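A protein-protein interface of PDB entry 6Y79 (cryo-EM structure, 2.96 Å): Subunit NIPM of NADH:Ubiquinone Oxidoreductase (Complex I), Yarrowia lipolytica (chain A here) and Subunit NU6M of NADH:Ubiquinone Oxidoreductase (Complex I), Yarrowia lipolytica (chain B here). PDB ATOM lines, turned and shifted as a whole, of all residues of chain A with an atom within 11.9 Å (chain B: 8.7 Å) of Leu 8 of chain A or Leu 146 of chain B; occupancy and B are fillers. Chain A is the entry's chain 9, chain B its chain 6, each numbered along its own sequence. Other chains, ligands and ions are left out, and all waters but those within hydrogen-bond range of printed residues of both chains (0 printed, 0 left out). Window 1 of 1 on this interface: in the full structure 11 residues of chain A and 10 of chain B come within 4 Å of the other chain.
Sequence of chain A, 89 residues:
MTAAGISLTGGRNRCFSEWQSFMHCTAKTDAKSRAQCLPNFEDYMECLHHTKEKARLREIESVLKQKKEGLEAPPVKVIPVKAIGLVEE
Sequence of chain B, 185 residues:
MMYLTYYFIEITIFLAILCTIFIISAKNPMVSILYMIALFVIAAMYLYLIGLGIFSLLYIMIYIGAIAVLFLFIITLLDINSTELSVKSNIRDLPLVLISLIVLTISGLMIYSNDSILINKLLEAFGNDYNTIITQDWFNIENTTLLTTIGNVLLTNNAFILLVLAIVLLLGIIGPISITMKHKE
The side-chain hydroxyl (OG1) of Thr 149 of chain B lies within hydrogen-bond range of the backbone carbonyl oxygen (O) of Leu 8 of chain A (2.8 Å).
The backbone NH of Gly 10 of chain A is in hydrogen-bond range of the side-chain hydroxyl of Thr 149 of chain B (3.4 Å).
The backbone carbonyl oxygen (O) of Thr 145 of chain B sits at hydrogen-bond distance from the side-chain hydroxyl (OG1) of Thr 149 of chain B.
The backbone NH (N) of Gly 11 of chain A lies within hydrogen-bond range of the side-chain hydroxyl (OG) of Ser 7 of chain A, 3.1 Å away.
The side-chain hydroxyl of Thr 9 of chain A sits close to the backbone NH of Gly 11 of chain A, at 3.4 Å.
Among the printed residues, merely in contact across the chains: Thr 9 of chain A with Thr 144 of chain B, Thr 9 of chain A with Thr 149 of chain B, Thr 9 of chain A with Asn 140 of chain B, Ser 7 of chain A with Thr 149 of chain B, Ala 3 of chain A with Val 153 of chain B, Leu 8 of chain A with Leu 146 of chain B, Leu 8 of chain A with Thr 145 of chain B, Ile 6 of chain A with Val 153 of chain B and Ile 6 of chain A with Thr 149 of chain B.
Of the printed residues of chain B, Ala 3 of chain A touches Val 153 (3.6 Å).
Of chain B, only Thr 149 (3.6 Å) comes within 4 Å of Ser 7 of chain A.
Printed residues of chain B within 4 Å of Thr 9 of chain A: Asn 140, Thr 144 and Thr 149.
Of the printed residues of chain B, Gly 10 of chain A touches Thr 149 (3.4 Å).
No residue of chain A comes within 4 Å of Leu 52 of chain B.
Phe 55 of chain B touches none of the printed residues of chain A.
Of chain A, only Thr 9 (3.3 Å) comes within 4 Å of Thr 144 of chain B.
Leu 146 of chain B touches just one residue of chain A: Leu 8.
No residue of chain A comes within 4 Å of Thr 148 of chain B.
Of chain A, only Ile 6 (3.8 Å), Ser 7 (3.6 Å), Leu 8 (2.8 Å), Thr 9 (3.6 Å) and Gly 10 (3.4 Å) come within 4 Å of Thr 149 of chain B.
Printed residues of chain A within 4 Å of Val 153 of chain B: Ala 3 and Ile 6.
The nearest residue of chain B that does not touch Leu 8 of chain A is Thr 144 of chain B (4.4 Å).
The nearest residue of chain A that does not touch Leu 146 of chain B is Thr 9 of chain A (6.0 Å).
Of the 14 printed residues of chain A, 6 touch a printed residue of chain B.
Hydrophobic or aromatic side chains of chain A within 4 Å of the printed part of chain B: Ala 3, Ile 6 and Leu 8.
Printed residues of chain B that touch a printed residue of chain A: Asn 140, Thr 144, Thr 145, Leu 146, Thr 149 and Val 153.
Hydrophobic or aromatic side chains of chain B that line the printed part of chain A: Leu 146 and Val 153.
Among the printed residues, no Asp or Glu carboxylate lies within 4 Å of a Lys or Arg side-chain nitrogen of the other chain.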
ATOM      1  N   ALA A   3       0.434  14.189 -20.513  1.00  0.00           N
ATOM      2  CA  ALA A   3       0.078  14.292 -19.107  1.00  0.00           C
ATOM      3  C   ALA A   3      -1.374  13.875 -18.906  1.00  0.00           C
ATOM      4  O   ALA A   3      -2.212  14.661 -18.478  1.00  0.00           O
ATOM      5  CB  ALA A   3       0.293  15.716 -18.618  1.00  0.00           C
ATOM      6  N   ALA A   4      -1.662  12.608 -19.194  1.00  0.00           N
ATOM      7  CA  ALA A   4      -3.048  12.155 -19.138  1.00  0.00           C
ATOM      8  C   ALA A   4      -3.518  11.990 -17.699  1.00  0.00           C
ATOM      9  O   ALA A   4      -4.550  12.545 -17.304  1.00  0.00           O
ATOM     10  CB  ALA A   4      -3.205  10.852 -19.917  1.00  0.00           C
ATOM     11  N   GLY A   5      -2.771  11.253 -16.890  1.00  0.00           N
ATOM     12  CA  GLY A   5      -3.201  11.040 -15.526  1.00  0.00           C
ATOM     13  C   GLY A   5      -2.213  11.504 -14.482  1.00  0.00           C
ATOM     14  O   GLY A   5      -2.187  10.963 -13.381  1.00  0.00           O
ATOM     15  N   ILE A   6      -1.399  12.496 -14.804  1.00  0.00           N
ATOM     16  CA  ILE A   6      -0.366  12.978 -13.898  1.00  0.00           C
ATOM     17  C   ILE A   6      -0.966  14.055 -13.011  1.00  0.00           C
ATOM     18  O   ILE A   6      -1.608  14.985 -13.504  1.00  0.00           O
ATOM     19  CB  ILE A   6       0.844  13.507 -14.682  1.00  0.00           C
ATOM     20  CG1 ILE A   6       1.312  12.450 -15.682  1.00  0.00           C
ATOM     21  CG2 ILE A   6       1.962  13.881 -13.742  1.00  0.00           C
ATOM     22  CD1 ILE A   6       2.452  12.885 -16.551  1.00  0.00           C
ATOM     23  N   SER A   7      -0.768  13.928 -11.702  1.00  0.00           N
ATOM     24  CA  SER A   7      -1.324  14.868 -10.742  1.00  0.00           C
ATOM     25  C   SER A   7      -0.302  15.953 -10.424  1.00  0.00           C
ATOM     26  O   SER A   7       0.792  15.982 -10.990  1.00  0.00           O
ATOM     27  CB  SER A   7      -1.762  14.142  -9.474  1.00  0.00           C
ATOM     28  OG  SER A   7      -0.653  13.683  -8.736  1.00  0.00           O
ATOM     29  N   LEU A   8      -0.654  16.840  -9.484  1.00  0.00           N
ATOM     30  CA  LEU A   8       0.198  17.971  -9.116  1.00  0.00           C
ATOM     31  C   LEU A   8       1.507  17.518  -8.492  1.00  0.00           C
ATOM     32  O   LEU A   8       2.537  18.178  -8.665  1.00  0.00           O
ATOM     33  CB  LEU A   8      -0.534  18.884  -8.133  1.00  0.00           C
ATOM     34  CG  LEU A   8      -1.477  19.999  -8.579  1.00  0.00           C
ATOM     35  CD1 LEU A   8      -2.789  19.423  -8.959  1.00  0.00           C
ATOM     36  CD2 LEU A   8      -1.688  20.972  -7.441  1.00  0.00           C
ATOM     37  N   THR A   9       1.493  16.403  -7.779  1.00  0.00           N
ATOM     38  CA  THR A   9       2.696  15.845  -7.192  1.00  0.00           C
ATOM     39  C   THR A   9       3.382  14.863  -8.116  1.00  0.00           C
ATOM     40  O   THR A   9       4.305  14.175  -7.684  1.00  0.00           O
ATOM     41  CB  THR A   9       2.369  15.144  -5.879  1.00  0.00           C
ATOM     42  OG1 THR A   9       1.863  13.831  -6.158  1.00  0.00           O
ATOM     43  CG2 THR A   9       1.320  15.930  -5.109  1.00  0.00           C
ATOM     44  N   GLY A  10       2.943  14.757  -9.361  1.00  0.00           N
ATOM     45  CA  GLY A  10       3.479  13.756 -10.244  1.00  0.00           C
ATOM     46  C   GLY A  10       2.880  12.388 -10.100  1.00  0.00           C
ATOM     47  O   GLY A  10       3.247  11.494 -10.865  1.00  0.00           O
ATOM     48  N   GLY A  11       1.987  12.188  -9.144  1.00  0.00           N
ATOM     49  CA  GLY A  11       1.297  10.930  -8.988  1.00  0.00           C
ATOM     50  C   GLY A  11       0.110  10.837  -9.920  1.00  0.00           C
ATOM     51  O   GLY A  11       0.019  11.538 -10.928  1.00  0.00           O
ATOM     52  N   ARG A  12      -0.815   9.956  -9.577  1.00  0.00           N
ATOM     53  CA  ARG A  12      -2.042   9.825 -10.344  1.00  0.00           C
ATOM     54  C   ARG A  12      -3.081  10.809  -9.819  1.00  0.00           C
ATOM     55  O   ARG A  12      -3.080  11.161  -8.638  1.00  0.00           O
ATOM     56  CB  ARG A  12      -2.550   8.386 -10.288  1.00  0.00           C
ATOM     57  CG  ARG A  12      -1.570   7.395 -10.890  1.00  0.00           C
ATOM     58  CD  ARG A  12      -1.800   5.995 -10.426  1.00  0.00           C
ATOM     59  NE  ARG A  12      -1.057   5.021 -11.210  1.00  0.00           N
ATOM     60  CZ  ARG A  12      -1.418   3.755 -11.376  1.00  0.00           C
ATOM     61  NH1 ARG A  12      -2.516   3.309 -10.809  1.00  0.00           N
ATOM     62  NH2 ARG A  12      -0.678   2.935 -12.113  1.00  0.00           N
ATOM     63  N   ASN A  13      -3.956  11.281 -10.706  1.00  0.00           N
ATOM     64  CA  ASN A  13      -4.878  12.338 -10.308  1.00  0.00           C
ATOM     65  C   ASN A  13      -6.042  11.746  -9.516  1.00  0.00           C
ATOM     66  O   ASN A  13      -6.059  10.563  -9.169  1.00  0.00           O
ATOM     67  CB  ASN A  13      -5.317  13.185 -11.510  1.00  0.00           C
ATOM     68  CG  ASN A  13      -5.903  12.397 -12.646  1.00  0.00           C
ATOM     69  OD1 ASN A  13      -6.238  11.241 -12.518  1.00  0.00           O
ATOM     70  ND2 ASN A  13      -6.052  13.052 -13.781  1.00  0.00           N
ATOM     71  N   ARG A  14      -7.024  12.585  -9.200  1.00  0.00           N
ATOM     72  CA  ARG A  14      -8.097  12.168  -8.309  1.00  0.00           C
ATOM     73  C   ARG A  14      -9.036  11.175  -8.979  1.00  0.00           C
ATOM     74  O   ARG A  14      -9.539  10.259  -8.322  1.00  0.00           O
ATOM     75  CB  ARG A  14      -8.862  13.392  -7.836  1.00  0.00           C
ATOM     76  CG  ARG A  14      -9.794  13.141  -6.698  1.00  0.00           C
ATOM     77  CD  ARG A  14     -10.564  14.392  -6.418  1.00  0.00           C
ATOM     78  NE  ARG A  14     -11.299  14.818  -7.598  1.00  0.00           N
ATOM     79  CZ  ARG A  14     -11.876  16.003  -7.717  1.00  0.00           C
ATOM     80  NH1 ARG A  14     -12.527  16.316  -8.823  1.00  0.00           N
ATOM     81  NH2 ARG A  14     -11.795  16.880  -6.725  1.00  0.00           N
ATOM     82  N   CYS A  15      -9.269  11.321 -10.278  1.00  0.00           N
ATOM     83  CA  CYS A  15     -10.162  10.440 -11.013  1.00  0.00           C
ATOM     84  C   CYS A  15      -9.409   9.497 -11.931  1.00  0.00           C
ATOM     85  O   CYS A  15      -9.909   9.141 -12.998  1.00  0.00           O
ATOM     86  CB  CYS A  15     -11.163  11.246 -11.824  1.00  0.00           C
ATOM     87  SG  CYS A  15     -12.291  12.163 -10.822  1.00  0.00           S
ATOM     88  N   PHE A  16      -8.200   9.106 -11.543  1.00  0.00           N
ATOM     89  CA  PHE A  16      -7.435   8.196 -12.378  1.00  0.00           C
ATOM     90  C   PHE A  16      -8.038   6.810 -12.392  1.00  0.00           C
ATOM     91  O   PHE A  16      -7.984   6.125 -13.418  1.00  0.00           O
ATOM     92  CB  PHE A  16      -5.992   8.107 -11.907  1.00  0.00           C
ATOM     93  CG  PHE A  16      -5.146   7.260 -12.777  1.00  0.00           C
ATOM     94  CD1 PHE A  16      -4.759   7.712 -14.019  1.00  0.00           C
ATOM     95  CD2 PHE A  16      -4.763   6.003 -12.374  1.00  0.00           C
ATOM     96  CE1 PHE A  16      -3.990   6.936 -14.830  1.00  0.00           C
ATOM     97  CE2 PHE A  16      -3.986   5.235 -13.182  1.00  0.00           C
ATOM     98  CZ  PHE A  16      -3.609   5.698 -14.410  1.00  0.00           C
ATOM     99  N   ILE B  50      -6.478  30.433  -3.902  1.00  0.00           N
ATOM    100  CA  ILE B  50      -6.987  29.120  -4.279  1.00  0.00           C
ATOM    101  C   ILE B  50      -6.003  28.001  -3.933  1.00  0.00           C
ATOM    102  O   ILE B  50      -6.417  26.852  -3.746  1.00  0.00           O
ATOM    103  CB  ILE B  50      -7.368  29.158  -5.771  1.00  0.00           C
ATOM    104  CG1 ILE B  50      -8.166  27.932  -6.182  1.00  0.00           C
ATOM    105  CG2 ILE B  50      -6.160  29.290  -6.659  1.00  0.00           C
ATOM    106  CD1 ILE B  50      -8.754  28.052  -7.529  1.00  0.00           C
ATOM    107  N   GLY B  51      -4.718  28.305  -3.790  1.00  0.00           N
ATOM    108  CA  GLY B  51      -3.761  27.299  -3.376  1.00  0.00           C
ATOM    109  C   GLY B  51      -2.520  27.247  -4.236  1.00  0.00           C
ATOM    110  O   GLY B  51      -1.629  26.429  -4.003  1.00  0.00           O
ATOM    111  N   LEU B  52      -2.463  28.107  -5.248  1.00  0.00           N
ATOM    112  CA  LEU B  52      -1.359  28.139  -6.204  1.00  0.00           C
ATOM    113  C   LEU B  52      -0.434  29.305  -5.877  1.00  0.00           C
ATOM    114  O   LEU B  52      -0.458  30.351  -6.518  1.00  0.00           O
ATOM    115  CB  LEU B  52      -1.902  28.247  -7.616  1.00  0.00           C
ATOM    116  CG  LEU B  52      -2.767  27.082  -8.067  1.00  0.00           C
ATOM    117  CD1 LEU B  52      -3.370  27.368  -9.411  1.00  0.00           C
ATOM    118  CD2 LEU B  52      -1.947  25.816  -8.117  1.00  0.00           C
ATOM    119  N   GLY B  53       0.406  29.113  -4.861  1.00  0.00           N
ATOM    120  CA  GLY B  53       1.347  30.156  -4.498  1.00  0.00           C
ATOM    121  C   GLY B  53       2.494  30.322  -5.471  1.00  0.00           C
ATOM    122  O   GLY B  53       3.102  31.396  -5.515  1.00  0.00           O
ATOM    123  N   ILE B  54       2.809  29.280  -6.241  1.00  0.00           N
ATOM    124  CA  ILE B  54       3.867  29.364  -7.246  1.00  0.00           C
ATOM    125  C   ILE B  54       3.459  30.312  -8.369  1.00  0.00           C
ATOM    126  O   ILE B  54       4.233  31.186  -8.794  1.00  0.00           O
ATOM    127  CB  ILE B  54       4.184  27.961  -7.797  1.00  0.00           C
ATOM    128  CG1 ILE B  54       4.659  27.008  -6.695  1.00  0.00           C
ATOM    129  CG2 ILE B  54       5.246  28.042  -8.863  1.00  0.00           C
ATOM    130  CD1 ILE B  54       3.641  25.991  -6.227  1.00  0.00           C
ATOM    131  N   PHE B  55       2.224  30.155  -8.855  1.00  0.00           N
ATOM    132  CA  PHE B  55       1.782  30.869 -10.046  1.00  0.00           C
ATOM    133  C   PHE B  55       1.697  32.357  -9.811  1.00  0.00           C
ATOM    134  O   PHE B  55       1.976  33.128 -10.724  1.00  0.00           O
ATOM    135  CB  PHE B  55       0.425  30.369 -10.511  1.00  0.00           C
ATOM    136  CG  PHE B  55       0.476  29.069 -11.215  1.00  0.00           C
ATOM    137  CD1 PHE B  55       1.013  28.967 -12.485  1.00  0.00           C
ATOM    138  CD2 PHE B  55      -0.026  27.945 -10.613  1.00  0.00           C
ATOM    139  CE1 PHE B  55       1.053  27.756 -13.126  1.00  0.00           C
ATOM    140  CE2 PHE B  55      -0.009  26.746 -11.248  1.00  0.00           C
ATOM    141  CZ  PHE B  55       0.545  26.643 -12.503  1.00  0.00           C
ATOM    142  N   SER B  56       1.311  32.772  -8.603  1.00  0.00           N
ATOM    143  CA  SER B  56       1.156  34.187  -8.283  1.00  0.00           C
ATOM    144  C   SER B  56       2.462  34.945  -8.449  1.00  0.00           C
ATOM    145  O   SER B  56       2.496  36.032  -9.039  1.00  0.00           O
ATOM    146  CB  SER B  56       0.638  34.328  -6.859  1.00  0.00           C
ATOM    147  OG  SER B  56       1.584  33.836  -5.932  1.00  0.00           O
ATOM    148  N   LEU B  58       4.875  33.777 -10.365  1.00  0.00           N
ATOM    149  CA  LEU B  58       5.133  33.734 -11.809  1.00  0.00           C
ATOM    150  C   LEU B  58       4.392  34.851 -12.555  1.00  0.00           C
ATOM    151  O   LEU B  58       4.920  35.408 -13.526  1.00  0.00           O
ATOM    152  CB  LEU B  58       4.765  32.364 -12.384  1.00  0.00           C
ATOM    153  CG  LEU B  58       5.844  31.280 -12.531  1.00  0.00           C
ATOM    154  CD1 LEU B  58       6.975  31.770 -13.386  1.00  0.00           C
ATOM    155  CD2 LEU B  58       6.390  30.794 -11.212  1.00  0.00           C
ATOM    156  N   ASN B 140       2.794   9.794  -0.535  1.00  0.00           N
ATOM    157  CA  ASN B 140       3.816  10.560  -1.241  1.00  0.00           C
ATOM    158  C   ASN B 140       4.974  10.881  -0.309  1.00  0.00           C
ATOM    159  O   ASN B 140       4.777  11.501   0.736  1.00  0.00           O
ATOM    160  CB  ASN B 140       3.228  11.854  -1.800  1.00  0.00           C
ATOM    161  CG  ASN B 140       4.195  12.591  -2.695  1.00  0.00           C
ATOM    162  OD1 ASN B 140       5.158  12.018  -3.202  1.00  0.00           O
ATOM    163  ND2 ASN B 140       3.951  13.879  -2.885  1.00  0.00           N
ATOM    164  N   ASN B 143       9.286  15.892  -1.771  1.00  0.00           N
ATOM    165  CA  ASN B 143       8.848  17.267  -1.997  1.00  0.00           C
ATOM    166  C   ASN B 143       8.769  17.553  -3.493  1.00  0.00           C
ATOM    167  O   ASN B 143       9.420  18.446  -4.037  1.00  0.00           O
ATOM    168  CB  ASN B 143       9.779  18.240  -1.289  1.00  0.00           C
ATOM    169  CG  ASN B 143       9.083  19.528  -0.888  1.00  0.00           C
ATOM    170  OD1 ASN B 143       7.859  19.634  -0.950  1.00  0.00           O
ATOM    171  ND2 ASN B 143       9.867  20.512  -0.466  1.00  0.00           N
ATOM    172  N   THR B 144       7.949  16.761  -4.166  1.00  0.00           N
ATOM    173  CA  THR B 144       7.552  17.107  -5.517  1.00  0.00           C
ATOM    174  C   THR B 144       6.440  18.130  -5.405  1.00  0.00           C
ATOM    175  O   THR B 144       5.277  17.786  -5.199  1.00  0.00           O
ATOM    176  CB  THR B 144       7.107  15.877  -6.291  1.00  0.00           C
ATOM    177  OG1 THR B 144       8.134  14.884  -6.240  1.00  0.00           O
ATOM    178  CG2 THR B 144       6.886  16.257  -7.727  1.00  0.00           C
ATOM    179  N   THR B 145       6.801  19.398  -5.503  1.00  0.00           N
ATOM    180  CA  THR B 145       5.786  20.424  -5.611  1.00  0.00           C
ATOM    181  C   THR B 145       5.428  20.615  -7.079  1.00  0.00           C
ATOM    182  O   THR B 145       5.831  19.846  -7.952  1.00  0.00           O
ATOM    183  CB  THR B 145       6.255  21.725  -4.967  1.00  0.00           C
ATOM    184  OG1 THR B 145       7.377  22.249  -5.685  1.00  0.00           O
ATOM    185  CG2 THR B 145       6.642  21.480  -3.526  1.00  0.00           C
ATOM    186  N   LEU B 146       4.669  21.668  -7.349  1.00  0.00           N
ATOM    187  CA  LEU B 146       4.022  21.814  -8.644  1.00  0.00           C
ATOM    188  C   LEU B 146       5.015  22.207  -9.733  1.00  0.00           C
ATOM    189  O   LEU B 146       4.882  21.780 -10.887  1.00  0.00           O
ATOM    190  CB  LEU B 146       2.901  22.835  -8.505  1.00  0.00           C
ATOM    191  CG  LEU B 146       2.016  23.201  -9.674  1.00  0.00           C
ATOM    192  CD1 LEU B 146       0.616  23.322  -9.176  1.00  0.00           C
ATOM    193  CD2 LEU B 146       2.482  24.521 -10.178  1.00  0.00           C
ATOM    194  N   LEU B 147       6.017  23.014  -9.382  1.00  0.00           N
ATOM    195  CA  LEU B 147       7.030  23.420 -10.348  1.00  0.00           C
ATOM    196  C   LEU B 147       7.911  22.246 -10.760  1.00  0.00           C
ATOM    197  O   LEU B 147       8.373  22.188 -11.905  1.00  0.00           O
ATOM    198  CB  LEU B 147       7.864  24.552  -9.758  1.00  0.00           C
ATOM    199  CG  LEU B 147       8.799  25.313 -10.687  1.00  0.00           C
ATOM    200  CD1 LEU B 147       8.018  25.959 -11.802  1.00  0.00           C
ATOM    201  CD2 LEU B 147       9.554  26.354  -9.901  1.00  0.00           C
ATOM    202  N   THR B 148       8.104  21.283  -9.858  1.00  0.00           N
ATOM    203  CA  THR B 148       8.837  20.070 -10.191  1.00  0.00           C
ATOM    204  C   THR B 148       8.092  19.225 -11.216  1.00  0.00           C
ATOM    205  O   THR B 148       8.697  18.708 -12.160  1.00  0.00           O
ATOM    206  CB  THR B 148       9.096  19.264  -8.922  1.00  0.00           C
ATOM    207  OG1 THR B 148       9.847  20.060  -8.001  1.00  0.00           O
ATOM    208  CG2 THR B 148       9.876  18.007  -9.240  1.00  0.00           C
ATOM    209  N   THR B 149       6.773  19.092 -11.070  1.00  0.00           N
ATOM    210  CA  THR B 149       6.042  18.262 -12.016  1.00  0.00           C
ATOM    211  C   THR B 149       5.862  18.977 -13.348  1.00  0.00           C
ATOM    212  O   THR B 149       5.841  18.320 -14.398  1.00  0.00           O
ATOM    213  CB  THR B 149       4.700  17.848 -11.426  1.00  0.00           C
ATOM    214  OG1 THR B 149       4.901  17.445 -10.072  1.00  0.00           O
ATOM    215  CG2 THR B 149       4.127  16.672 -12.216  1.00  0.00           C
ATOM    216  N   ILE B 150       5.769  20.313 -13.336  1.00  0.00           N
ATOM    217  CA  ILE B 150       5.801  21.061 -14.593  1.00  0.00           C
ATOM    218  C   ILE B 150       7.137  20.855 -15.297  1.00  0.00           C
ATOM    219  O   ILE B 150       7.191  20.642 -16.513  1.00  0.00           O
ATOM    220  CB  ILE B 150       5.502  22.554 -14.355  1.00  0.00           C
ATOM    221  CG1 ILE B 150       4.047  22.741 -13.948  1.00  0.00           C
ATOM    222  CG2 ILE B 150       5.727  23.360 -15.611  1.00  0.00           C
ATOM    223  CD1 ILE B 150       3.677  24.174 -13.674  1.00  0.00           C
ATOM    224  N   GLY B 151       8.228  20.839 -14.538  1.00  0.00           N
ATOM    225  CA  GLY B 151       9.505  20.512 -15.134  1.00  0.00           C
ATOM    226  C   GLY B 151       9.687  19.059 -15.521  1.00  0.00           C
ATOM    227  O   GLY B 151      10.596  18.767 -16.299  1.00  0.00           O
ATOM    228  N   ASN B 152       8.900  18.138 -14.977  1.00  0.00           N
ATOM    229  CA  ASN B 152       9.002  16.763 -15.452  1.00  0.00           C
ATOM    230  C   ASN B 152       8.235  16.571 -16.740  1.00  0.00           C
ATOM    231  O   ASN B 152       8.703  15.866 -17.634  1.00  0.00           O
ATOM    232  CB  ASN B 152       8.475  15.780 -14.398  1.00  0.00           C
ATOM    233  CG  ASN B 152       8.844  14.319 -14.678  1.00  0.00           C
ATOM    234  OD1 ASN B 152       9.552  14.002 -15.634  1.00  0.00           O
ATOM    235  ND2 ASN B 152       8.315  13.414 -13.858  1.00  0.00           N
ATOM    236  N   VAL B 153       7.098  17.234 -16.890  1.00  0.00           N
ATOM    237  CA  VAL B 153       6.239  16.926 -18.021  1.00  0.00           C
ATOM    238  C   VAL B 153       6.451  17.880 -19.200  1.00  0.00           C
ATOM    239  O   VAL B 153       6.240  17.489 -20.348  1.00  0.00           O
ATOM    240  CB  VAL B 153       4.795  16.885 -17.512  1.00  0.00           C
ATOM    241  CG1 VAL B 153       3.879  16.365 -18.549  1.00  0.00           C
ATOM    242  CG2 VAL B 153       4.762  15.913 -16.380  1.00  0.00           C
ATOM    243  N   LEU B 154       6.971  19.089 -18.969  1.00  0.00           N
ATOM    244  CA  LEU B 154       7.532  19.862 -20.075  1.00  0.00           C
ATOM    245  C   LEU B 154       8.749  19.198 -20.695  1.00  0.00           C
ATOM    246  O   LEU B 154       9.095  19.512 -21.835  1.00  0.00           O
ATOM    247  CB  LEU B 154       7.961  21.253 -19.623  1.00  0.00           C
ATOM    248  CG  LEU B 154       6.991  22.409 -19.471  1.00  0.00           C
ATOM    249  CD1 LEU B 154       7.740  23.566 -18.842  1.00  0.00           C
ATOM    250  CD2 LEU B 154       6.437  22.795 -20.818  1.00  0.00           C
